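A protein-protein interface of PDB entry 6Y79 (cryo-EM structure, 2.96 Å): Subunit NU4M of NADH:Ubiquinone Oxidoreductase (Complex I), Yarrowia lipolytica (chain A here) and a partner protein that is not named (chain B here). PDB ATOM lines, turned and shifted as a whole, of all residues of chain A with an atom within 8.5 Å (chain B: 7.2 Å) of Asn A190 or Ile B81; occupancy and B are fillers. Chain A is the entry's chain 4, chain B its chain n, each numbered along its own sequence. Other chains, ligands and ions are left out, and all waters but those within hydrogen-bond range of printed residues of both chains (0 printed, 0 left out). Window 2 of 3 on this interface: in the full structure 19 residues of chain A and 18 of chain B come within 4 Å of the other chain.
The backbone carbonyl oxygen (O) of Gln B76 sits at hydrogen-bond distance from the side-chain hydroxyl (OG1) of Thr B80.
Leu B73 touches Ser A74.
Gln B76 touches Ser A74.
O of Asn A190 touches CG of Arg B77, 3.7 Å away.
ND2 of Asn A190 touches CG1 of Ile B81 (3.4 Å).
Asn A193 touches Leu B73.
The backbone carbonyl oxygen of Leu A189 is in hydrogen-bond range of the guanidinium group of Arg B77 (2.7 Å).
Asn A190 touches just these residues of chain B: Arg B77 (3.7 Å) and Ile B81 (3.4 Å).
Printed residues of chain B within 4 Å of Asn A193: Leu B73.
Of the printed residues of chain A, Leu B73 touches Ser A74 (3.3 Å) and Asn A193 (3.4 Å).
Of the printed residues of chain A, Gln B76 touches Ser A74.
Printed residues of chain A within 4 Å of Arg B77: Leu A189 (2.7 Å) and Asn A190 (3.7 Å).
Ile B81 touches one residue of chain A.
Lys B82 touches none of the printed residues of chain A.
The nearest residue of chain B that does not touch Asn A190 is Thr B80 (4.2 Å).
The nearest residue of chain A that does not touch Ile B81 is Leu A189 (5.3 Å).
Along chain A the printed residues that touch a printed residue of chain B span positions 74 to 193.
Among the printed residues, 6 pairs touch across the chains.
Among the printed residues, no Asp or Glu carboxylate lies within 4 Å of a Lys or Arg side-chain nitrogen of the other chain.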
ATOM      1  N   SER A  74      22.658   1.548  -3.401  1.00  0.00           N
ATOM      2  CA  SER A  74      22.378   2.901  -3.843  1.00  0.00           C
ATOM      3  C   SER A  74      20.968   2.960  -4.385  1.00  0.00           C
ATOM      4  O   SER A  74      20.661   2.314  -5.390  1.00  0.00           O
ATOM      5  CB  SER A  74      23.376   3.347  -4.899  1.00  0.00           C
ATOM      6  OG  SER A  74      23.228   2.564  -6.063  1.00  0.00           O
ATOM      7  N   ILE A 182       8.561   6.249 -18.680  1.00  0.00           N
ATOM      8  CA  ILE A 182       9.572   6.110 -17.632  1.00  0.00           C
ATOM      9  C   ILE A 182       9.137   5.085 -16.586  1.00  0.00           C
ATOM     10  O   ILE A 182       9.951   4.290 -16.098  1.00  0.00           O
ATOM     11  CB  ILE A 182       9.881   7.491 -17.014  1.00  0.00           C
ATOM     12  CG1 ILE A 182      10.737   8.312 -17.973  1.00  0.00           C
ATOM     13  CG2 ILE A 182      10.603   7.390 -15.688  1.00  0.00           C
ATOM     14  CD1 ILE A 182      11.026   9.694 -17.496  1.00  0.00           C
ATOM     15  N   VAL A 183       7.839   5.043 -16.274  1.00  0.00           N
ATOM     16  CA  VAL A 183       7.311   4.049 -15.338  1.00  0.00           C
ATOM     17  C   VAL A 183       7.405   2.645 -15.926  1.00  0.00           C
ATOM     18  O   VAL A 183       7.768   1.690 -15.224  1.00  0.00           O
ATOM     19  CB  VAL A 183       5.866   4.413 -14.948  1.00  0.00           C
ATOM     20  CG1 VAL A 183       5.176   3.276 -14.249  1.00  0.00           C
ATOM     21  CG2 VAL A 183       5.866   5.581 -14.038  1.00  0.00           C
ATOM     22  N   VAL A 184       7.113   2.498 -17.221  1.00  0.00           N
ATOM     23  CA  VAL A 184       7.234   1.186 -17.857  1.00  0.00           C
ATOM     24  C   VAL A 184       8.686   0.715 -17.872  1.00  0.00           C
ATOM     25  O   VAL A 184       8.971  -0.456 -17.587  1.00  0.00           O
ATOM     26  CB  VAL A 184       6.622   1.221 -19.266  1.00  0.00           C
ATOM     27  CG1 VAL A 184       6.827  -0.091 -19.983  1.00  0.00           C
ATOM     28  CG2 VAL A 184       5.167   1.498 -19.151  1.00  0.00           C
ATOM     29  N   ILE A 185       9.627   1.629 -18.138  1.00  0.00           N
ATOM     30  CA  ILE A 185      11.051   1.297 -18.069  1.00  0.00           C
ATOM     31  C   ILE A 185      11.446   0.878 -16.656  1.00  0.00           C
ATOM     32  O   ILE A 185      12.145  -0.122 -16.465  1.00  0.00           O
ATOM     33  CB  ILE A 185      11.900   2.483 -18.568  1.00  0.00           C
ATOM     34  CG1 ILE A 185      11.752   2.666 -20.072  1.00  0.00           C
ATOM     35  CG2 ILE A 185      13.362   2.281 -18.281  1.00  0.00           C
ATOM     36  CD1 ILE A 185      12.353   3.949 -20.569  1.00  0.00           C
ATOM     37  N   SER A 186      10.963   1.594 -15.643  1.00  0.00           N
ATOM     38  CA  SER A 186      11.340   1.288 -14.266  1.00  0.00           C
ATOM     39  C   SER A 186      10.664   0.050 -13.704  1.00  0.00           C
ATOM     40  O   SER A 186      11.105  -0.442 -12.665  1.00  0.00           O
ATOM     41  CB  SER A 186      11.020   2.461 -13.343  1.00  0.00           C
ATOM     42  OG  SER A 186       9.634   2.683 -13.244  1.00  0.00           O
ATOM     43  N   ILE A 187       9.596  -0.449 -14.319  1.00  0.00           N
ATOM     44  CA  ILE A 187       9.022  -1.705 -13.849  1.00  0.00           C
ATOM     45  C   ILE A 187       9.483  -2.912 -14.662  1.00  0.00           C
ATOM     46  O   ILE A 187       9.402  -4.041 -14.159  1.00  0.00           O
ATOM     47  CB  ILE A 187       7.479  -1.660 -13.793  1.00  0.00           C
ATOM     48  CG1 ILE A 187       6.872  -1.526 -15.186  1.00  0.00           C
ATOM     49  CG2 ILE A 187       7.009  -0.557 -12.873  1.00  0.00           C
ATOM     50  CD1 ILE A 187       5.382  -1.601 -15.195  1.00  0.00           C
ATOM     51  N   VAL A 188       9.963  -2.718 -15.888  1.00  0.00           N
ATOM     52  CA  VAL A 188      10.602  -3.822 -16.602  1.00  0.00           C
ATOM     53  C   VAL A 188      12.017  -4.035 -16.096  1.00  0.00           C
ATOM     54  O   VAL A 188      12.408  -5.146 -15.722  1.00  0.00           O
ATOM     55  CB  VAL A 188      10.608  -3.570 -18.115  1.00  0.00           C
ATOM     56  CG1 VAL A 188      11.315  -4.689 -18.817  1.00  0.00           C
ATOM     57  CG2 VAL A 188       9.240  -3.491 -18.611  1.00  0.00           C
ATOM     58  N   LEU A 189      12.809  -2.972 -16.093  1.00  0.00           N
ATOM     59  CA  LEU A 189      14.228  -3.099 -15.815  1.00  0.00           C
ATOM     60  C   LEU A 189      14.516  -3.141 -14.327  1.00  0.00           C
ATOM     61  O   LEU A 189      15.544  -3.693 -13.923  1.00  0.00           O
ATOM     62  CB  LEU A 189      14.984  -1.933 -16.447  1.00  0.00           C
ATOM     63  CG  LEU A 189      14.947  -1.799 -17.961  1.00  0.00           C
ATOM     64  CD1 LEU A 189      15.768  -0.603 -18.379  1.00  0.00           C
ATOM     65  CD2 LEU A 189      15.492  -3.044 -18.573  1.00  0.00           C
ATOM     66  N   ASN A 190      13.642  -2.535 -13.518  1.00  0.00           N
ATOM     67  CA  ASN A 190      13.832  -2.261 -12.089  1.00  0.00           C
ATOM     68  C   ASN A 190      15.096  -1.459 -11.808  1.00  0.00           C
ATOM     69  O   ASN A 190      15.626  -1.498 -10.695  1.00  0.00           O
ATOM     70  CB  ASN A 190      13.810  -3.544 -11.254  1.00  0.00           C
ATOM     71  CG  ASN A 190      12.482  -4.243 -11.321  1.00  0.00           C
ATOM     72  OD1 ASN A 190      11.448  -3.654 -11.029  1.00  0.00           O
ATOM     73  ND2 ASN A 190      12.494  -5.498 -11.725  1.00  0.00           N
ATOM     74  N   THR A 191      15.561  -0.711 -12.805  1.00  0.00           N
ATOM     75  CA  THR A 191      16.692   0.196 -12.686  1.00  0.00           C
ATOM     76  C   THR A 191      16.411   1.367 -13.617  1.00  0.00           C
ATOM     77  O   THR A 191      15.876   1.174 -14.710  1.00  0.00           O
ATOM     78  CB  THR A 191      18.037  -0.512 -13.009  1.00  0.00           C
ATOM     79  OG1 THR A 191      19.126   0.400 -12.830  1.00  0.00           O
ATOM     80  CG2 THR A 191      18.089  -1.128 -14.423  1.00  0.00           C
ATOM     81  N   THR A 192      16.654   2.584 -13.141  1.00  0.00           N
ATOM     82  CA  THR A 192      16.691   3.770 -13.989  1.00  0.00           C
ATOM     83  C   THR A 192      18.047   4.422 -13.823  1.00  0.00           C
ATOM     84  O   THR A 192      18.412   4.827 -12.724  1.00  0.00           O
ATOM     85  CB  THR A 192      15.563   4.761 -13.666  1.00  0.00           C
ATOM     86  OG1 THR A 192      15.718   5.312 -12.357  1.00  0.00           O
ATOM     87  CG2 THR A 192      14.202   4.123 -13.811  1.00  0.00           C
ATOM     88  N   ASN A 193      18.785   4.516 -14.911  1.00  0.00           N
ATOM     89  CA  ASN A 193      20.218   4.725 -14.820  1.00  0.00           C
ATOM     90  C   ASN A 193      20.702   5.148 -16.193  1.00  0.00           C
ATOM     91  O   ASN A 193      20.259   4.590 -17.192  1.00  0.00           O
ATOM     92  CB  ASN A 193      20.898   3.423 -14.373  1.00  0.00           C
ATOM     93  CG  ASN A 193      22.355   3.584 -14.082  1.00  0.00           C
ATOM     94  OD1 ASN A 193      22.849   4.686 -13.889  1.00  0.00           O
ATOM     95  ND2 ASN A 193      23.071   2.470 -14.079  1.00  0.00           N
ATOM     96  N   PHE A 200      20.918  -3.372 -21.445  1.00  0.00           N
ATOM     97  CA  PHE A 200      19.631  -4.044 -21.442  1.00  0.00           C
ATOM     98  C   PHE A 200      18.994  -3.983 -22.822  1.00  0.00           C
ATOM     99  O   PHE A 200      18.976  -2.931 -23.461  1.00  0.00           O
ATOM    100  CB  PHE A 200      18.712  -3.387 -20.416  1.00  0.00           C
ATOM    101  CG  PHE A 200      19.207  -3.488 -19.000  1.00  0.00           C
ATOM    102  CD1 PHE A 200      18.957  -4.616 -18.247  1.00  0.00           C
ATOM    103  CD2 PHE A 200      19.919  -2.460 -18.424  1.00  0.00           C
ATOM    104  CE1 PHE A 200      19.398  -4.718 -16.951  1.00  0.00           C
ATOM    105  CE2 PHE A 200      20.372  -2.561 -17.124  1.00  0.00           C
ATOM    106  CZ  PHE A 200      20.107  -3.693 -16.390  1.00  0.00           C
ATOM    107  N   LEU B  73      24.271  -0.269  -7.885  1.00  0.00           N
ATOM    108  CA  LEU B  73      22.949  -0.175  -8.492  1.00  0.00           C
ATOM    109  C   LEU B  73      22.382  -1.529  -8.877  1.00  0.00           C
ATOM    110  O   LEU B  73      21.165  -1.731  -8.804  1.00  0.00           O
ATOM    111  CB  LEU B  73      22.999   0.709  -9.733  1.00  0.00           C
ATOM    112  CG  LEU B  73      23.159   2.202  -9.505  1.00  0.00           C
ATOM    113  CD1 LEU B  73      23.647   2.801 -10.777  1.00  0.00           C
ATOM    114  CD2 LEU B  73      21.847   2.822  -9.102  1.00  0.00           C
ATOM    115  N   ASN B  75      23.047  -4.139  -7.102  1.00  0.00           N
ATOM    116  CA  ASN B  75      22.627  -4.628  -5.794  1.00  0.00           C
ATOM    117  C   ASN B  75      21.221  -4.162  -5.454  1.00  0.00           C
ATOM    118  O   ASN B  75      20.410  -4.942  -4.947  1.00  0.00           O
ATOM    119  CB  ASN B  75      23.602  -4.168  -4.717  1.00  0.00           C
ATOM    120  CG  ASN B  75      24.900  -4.925  -4.750  1.00  0.00           C
ATOM    121  OD1 ASN B  75      24.937  -6.104  -5.084  1.00  0.00           O
ATOM    122  ND2 ASN B  75      25.980  -4.250  -4.395  1.00  0.00           N
ATOM    123  N   GLN B  76      20.909  -2.899  -5.741  1.00  0.00           N
ATOM    124  CA  GLN B  76      19.564  -2.386  -5.512  1.00  0.00           C
ATOM    125  C   GLN B  76      18.551  -3.017  -6.456  1.00  0.00           C
ATOM    126  O   GLN B  76      17.403  -3.247  -6.063  1.00  0.00           O
ATOM    127  CB  GLN B  76      19.560  -0.868  -5.655  1.00  0.00           C
ATOM    128  CG  GLN B  76      18.230  -0.199  -5.386  1.00  0.00           C
ATOM    129  CD  GLN B  76      17.765  -0.369  -3.961  1.00  0.00           C
ATOM    130  OE1 GLN B  76      18.548  -0.254  -3.020  1.00  0.00           O
ATOM    131  NE2 GLN B  76      16.480  -0.639  -3.790  1.00  0.00           N
ATOM    132  N   ARG B  77      18.958  -3.339  -7.681  1.00  0.00           N
ATOM    133  CA  ARG B  77      18.050  -4.021  -8.597  1.00  0.00           C
ATOM    134  C   ARG B  77      17.747  -5.443  -8.131  1.00  0.00           C
ATOM    135  O   ARG B  77      16.589  -5.882  -8.169  1.00  0.00           O
ATOM    136  CB  ARG B  77      18.633  -4.024 -10.003  1.00  0.00           C
ATOM    137  CG  ARG B  77      17.688  -4.574 -11.029  1.00  0.00           C
ATOM    138  CD  ARG B  77      18.379  -4.829 -12.328  1.00  0.00           C
ATOM    139  NE  ARG B  77      17.475  -5.460 -13.269  1.00  0.00           N
ATOM    140  CZ  ARG B  77      17.374  -6.770 -13.426  1.00  0.00           C
ATOM    141  NH1 ARG B  77      18.129  -7.579 -12.703  1.00  0.00           N
ATOM    142  NH2 ARG B  77      16.519  -7.269 -14.303  1.00  0.00           N
ATOM    143  N   GLU B  78      18.775  -6.172  -7.676  1.00  0.00           N
ATOM    144  CA  GLU B  78      18.575  -7.498  -7.094  1.00  0.00           C
ATOM    145  C   GLU B  78      17.712  -7.445  -5.843  1.00  0.00           C
ATOM    146  O   GLU B  78      16.846  -8.308  -5.654  1.00  0.00           O
ATOM    147  CB  GLU B  78      19.911  -8.137  -6.729  1.00  0.00           C
ATOM    148  CG  GLU B  78      20.801  -8.536  -7.874  1.00  0.00           C
ATOM    149  CD  GLU B  78      22.261  -8.571  -7.454  1.00  0.00           C
ATOM    150  OE1 GLU B  78      22.525  -8.694  -6.239  1.00  0.00           O
ATOM    151  OE2 GLU B  78      23.141  -8.461  -8.331  1.00  0.00           O
ATOM    152  N   LEU B  79      17.934  -6.439  -4.991  1.00  0.00           N
ATOM    153  CA  LEU B  79      17.136  -6.269  -3.783  1.00  0.00           C
ATOM    154  C   LEU B  79      15.678  -5.986  -4.113  1.00  0.00           C
ATOM    155  O   LEU B  79      14.770  -6.510  -3.461  1.00  0.00           O
ATOM    156  CB  LEU B  79      17.708  -5.136  -2.936  1.00  0.00           C
ATOM    157  CG  LEU B  79      16.947  -4.925  -1.630  1.00  0.00           C
ATOM    158  CD1 LEU B  79      17.167  -6.110  -0.708  1.00  0.00           C
ATOM    159  CD2 LEU B  79      17.287  -3.611  -0.953  1.00  0.00           C
ATOM    160  N   THR B  80      15.434  -5.172  -5.138  1.00  0.00           N
ATOM    161  CA  THR B  80      14.066  -4.832  -5.513  1.00  0.00           C
ATOM    162  C   THR B  80      13.333  -6.035  -6.100  1.00  0.00           C
ATOM    163  O   THR B  80      12.169  -6.286  -5.763  1.00  0.00           O
ATOM    164  CB  THR B  80      14.086  -3.661  -6.496  1.00  0.00           C
ATOM    165  OG1 THR B  80      14.625  -2.509  -5.844  1.00  0.00           O
ATOM    166  CG2 THR B  80      12.697  -3.330  -6.982  1.00  0.00           C
ATOM    167  N   ILE B  81      14.012  -6.812  -6.953  1.00  0.00           N
ATOM    168  CA  ILE B  81      13.398  -8.010  -7.526  1.00  0.00           C
ATOM    169  C   ILE B  81      13.123  -9.034  -6.434  1.00  0.00           C
ATOM    170  O   ILE B  81      12.077  -9.710  -6.434  1.00  0.00           O
ATOM    171  CB  ILE B  81      14.295  -8.586  -8.637  1.00  0.00           C
ATOM    172  CG1 ILE B  81      14.371  -7.604  -9.801  1.00  0.00           C
ATOM    173  CG2 ILE B  81      13.776  -9.905  -9.167  1.00  0.00           C
ATOM    174  CD1 ILE B  81      15.303  -8.034 -10.862  1.00  0.00           C
ATOM    175  N   LYS B  82      14.011  -9.099  -5.435  1.00  0.00           N
ATOM    176  CA  LYS B  82      13.798  -9.993  -4.303  1.00  0.00           C
ATOM    177  C   LYS B  82      12.582  -9.584  -3.480  1.00  0.00           C
ATOM    178  O   LYS B  82      11.653 -10.372  -3.315  1.00  0.00           O
ATOM    179  CB  LYS B  82      15.050 -10.023  -3.439  1.00  0.00           C
ATOM    180  CG  LYS B  82      15.083 -11.228  -2.550  1.00  0.00           C
ATOM    181  CD  LYS B  82      15.851 -10.969  -1.294  1.00  0.00           C
ATOM    182  CE  LYS B  82      17.327 -10.807  -1.564  1.00  0.00           C
ATOM    183  NZ  LYS B  82      18.093 -10.753  -0.288  1.00  0.00           N
ATOM    184  N   MET B  83      12.535  -8.325  -3.036  1.00  0.00           N
ATOM    185  CA  MET B  83      11.424  -7.829  -2.232  1.00  0.00           C
ATOM    186  C   MET B  83      10.101  -7.836  -2.990  1.00  0.00           C
ATOM    187  O   MET B  83       9.043  -7.825  -2.355  1.00  0.00           O
ATOM    188  CB  MET B  83      11.716  -6.441  -1.707  1.00  0.00           C
ATOM    189  CG  MET B  83      12.933  -6.325  -0.800  1.00  0.00           C
ATOM    190  SD  MET B  83      13.002  -7.573   0.490  1.00  0.00           S
ATOM    191  CE  MET B  83      11.724  -6.993   1.585  1.00  0.00           C
ATOM    192  N   HIS B  84      10.128  -7.857  -4.327  1.00  0.00           N
ATOM    193  CA  HIS B  84       8.912  -8.154  -5.073  1.00  0.00           C
ATOM    194  C   HIS B  84       8.548  -9.632  -5.017  1.00  0.00           C
ATOM    195  O   HIS B  84       7.357  -9.948  -4.956  1.00  0.00           O
ATOM    196  CB  HIS B  84       9.043  -7.721  -6.533  1.00  0.00           C
ATOM    197  CG  HIS B  84       8.980  -6.240  -6.740  1.00  0.00           C
ATOM    198  ND1 HIS B  84       8.056  -5.433  -6.112  1.00  0.00           N
ATOM    199  CD2 HIS B  84       9.725  -5.420  -7.516  1.00  0.00           C
ATOM    200  CE1 HIS B  84       8.244  -4.179  -6.482  1.00  0.00           C
ATOM    201  NE2 HIS B  84       9.253  -4.144  -7.333  1.00  0.00           N
ATOM    202  N   GLU B  85       9.537 -10.541  -5.078  1.00  0.00           N
ATOM    203  CA  GLU B  85       9.256 -11.976  -4.924  1.00  0.00           C
ATOM    204  C   GLU B  85       8.637 -12.284  -3.567  1.00  0.00           C
ATOM    205  O   GLU B  85       7.769 -13.154  -3.449  1.00  0.00           O
ATOM    206  CB  GLU B  85      10.534 -12.800  -5.024  1.00  0.00           C
ATOM    207  CG  GLU B  85      11.166 -13.053  -6.357  1.00  0.00           C
ATOM    208  CD  GLU B  85      12.519 -13.736  -6.163  1.00  0.00           C
ATOM    209  OE1 GLU B  85      12.549 -14.820  -5.540  1.00  0.00           O
ATOM    210  OE2 GLU B  85      13.550 -13.189  -6.610  1.00  0.00           O
ATOM    211  N   LEU B  86       9.121 -11.612  -2.528  1.00  0.00           N
ATOM    212  CA  LEU B  86       8.763 -11.944  -1.152  1.00  0.00           C
ATOM    213  C   LEU B  86       7.311 -11.665  -0.812  1.00  0.00           C
ATOM    214  O   LEU B  86       6.779 -12.286   0.112  1.00  0.00           O
ATOM    215  CB  LEU B  86       9.642 -11.177  -0.174  1.00  0.00           C
ATOM    216  CG  LEU B  86      10.869 -11.833   0.464  1.00  0.00           C
ATOM    217  CD1 LEU B  86      11.938 -12.193  -0.628  1.00  0.00           C
ATOM    218  CD2 LEU B  86      11.461 -10.899   1.547  1.00  0.00           C
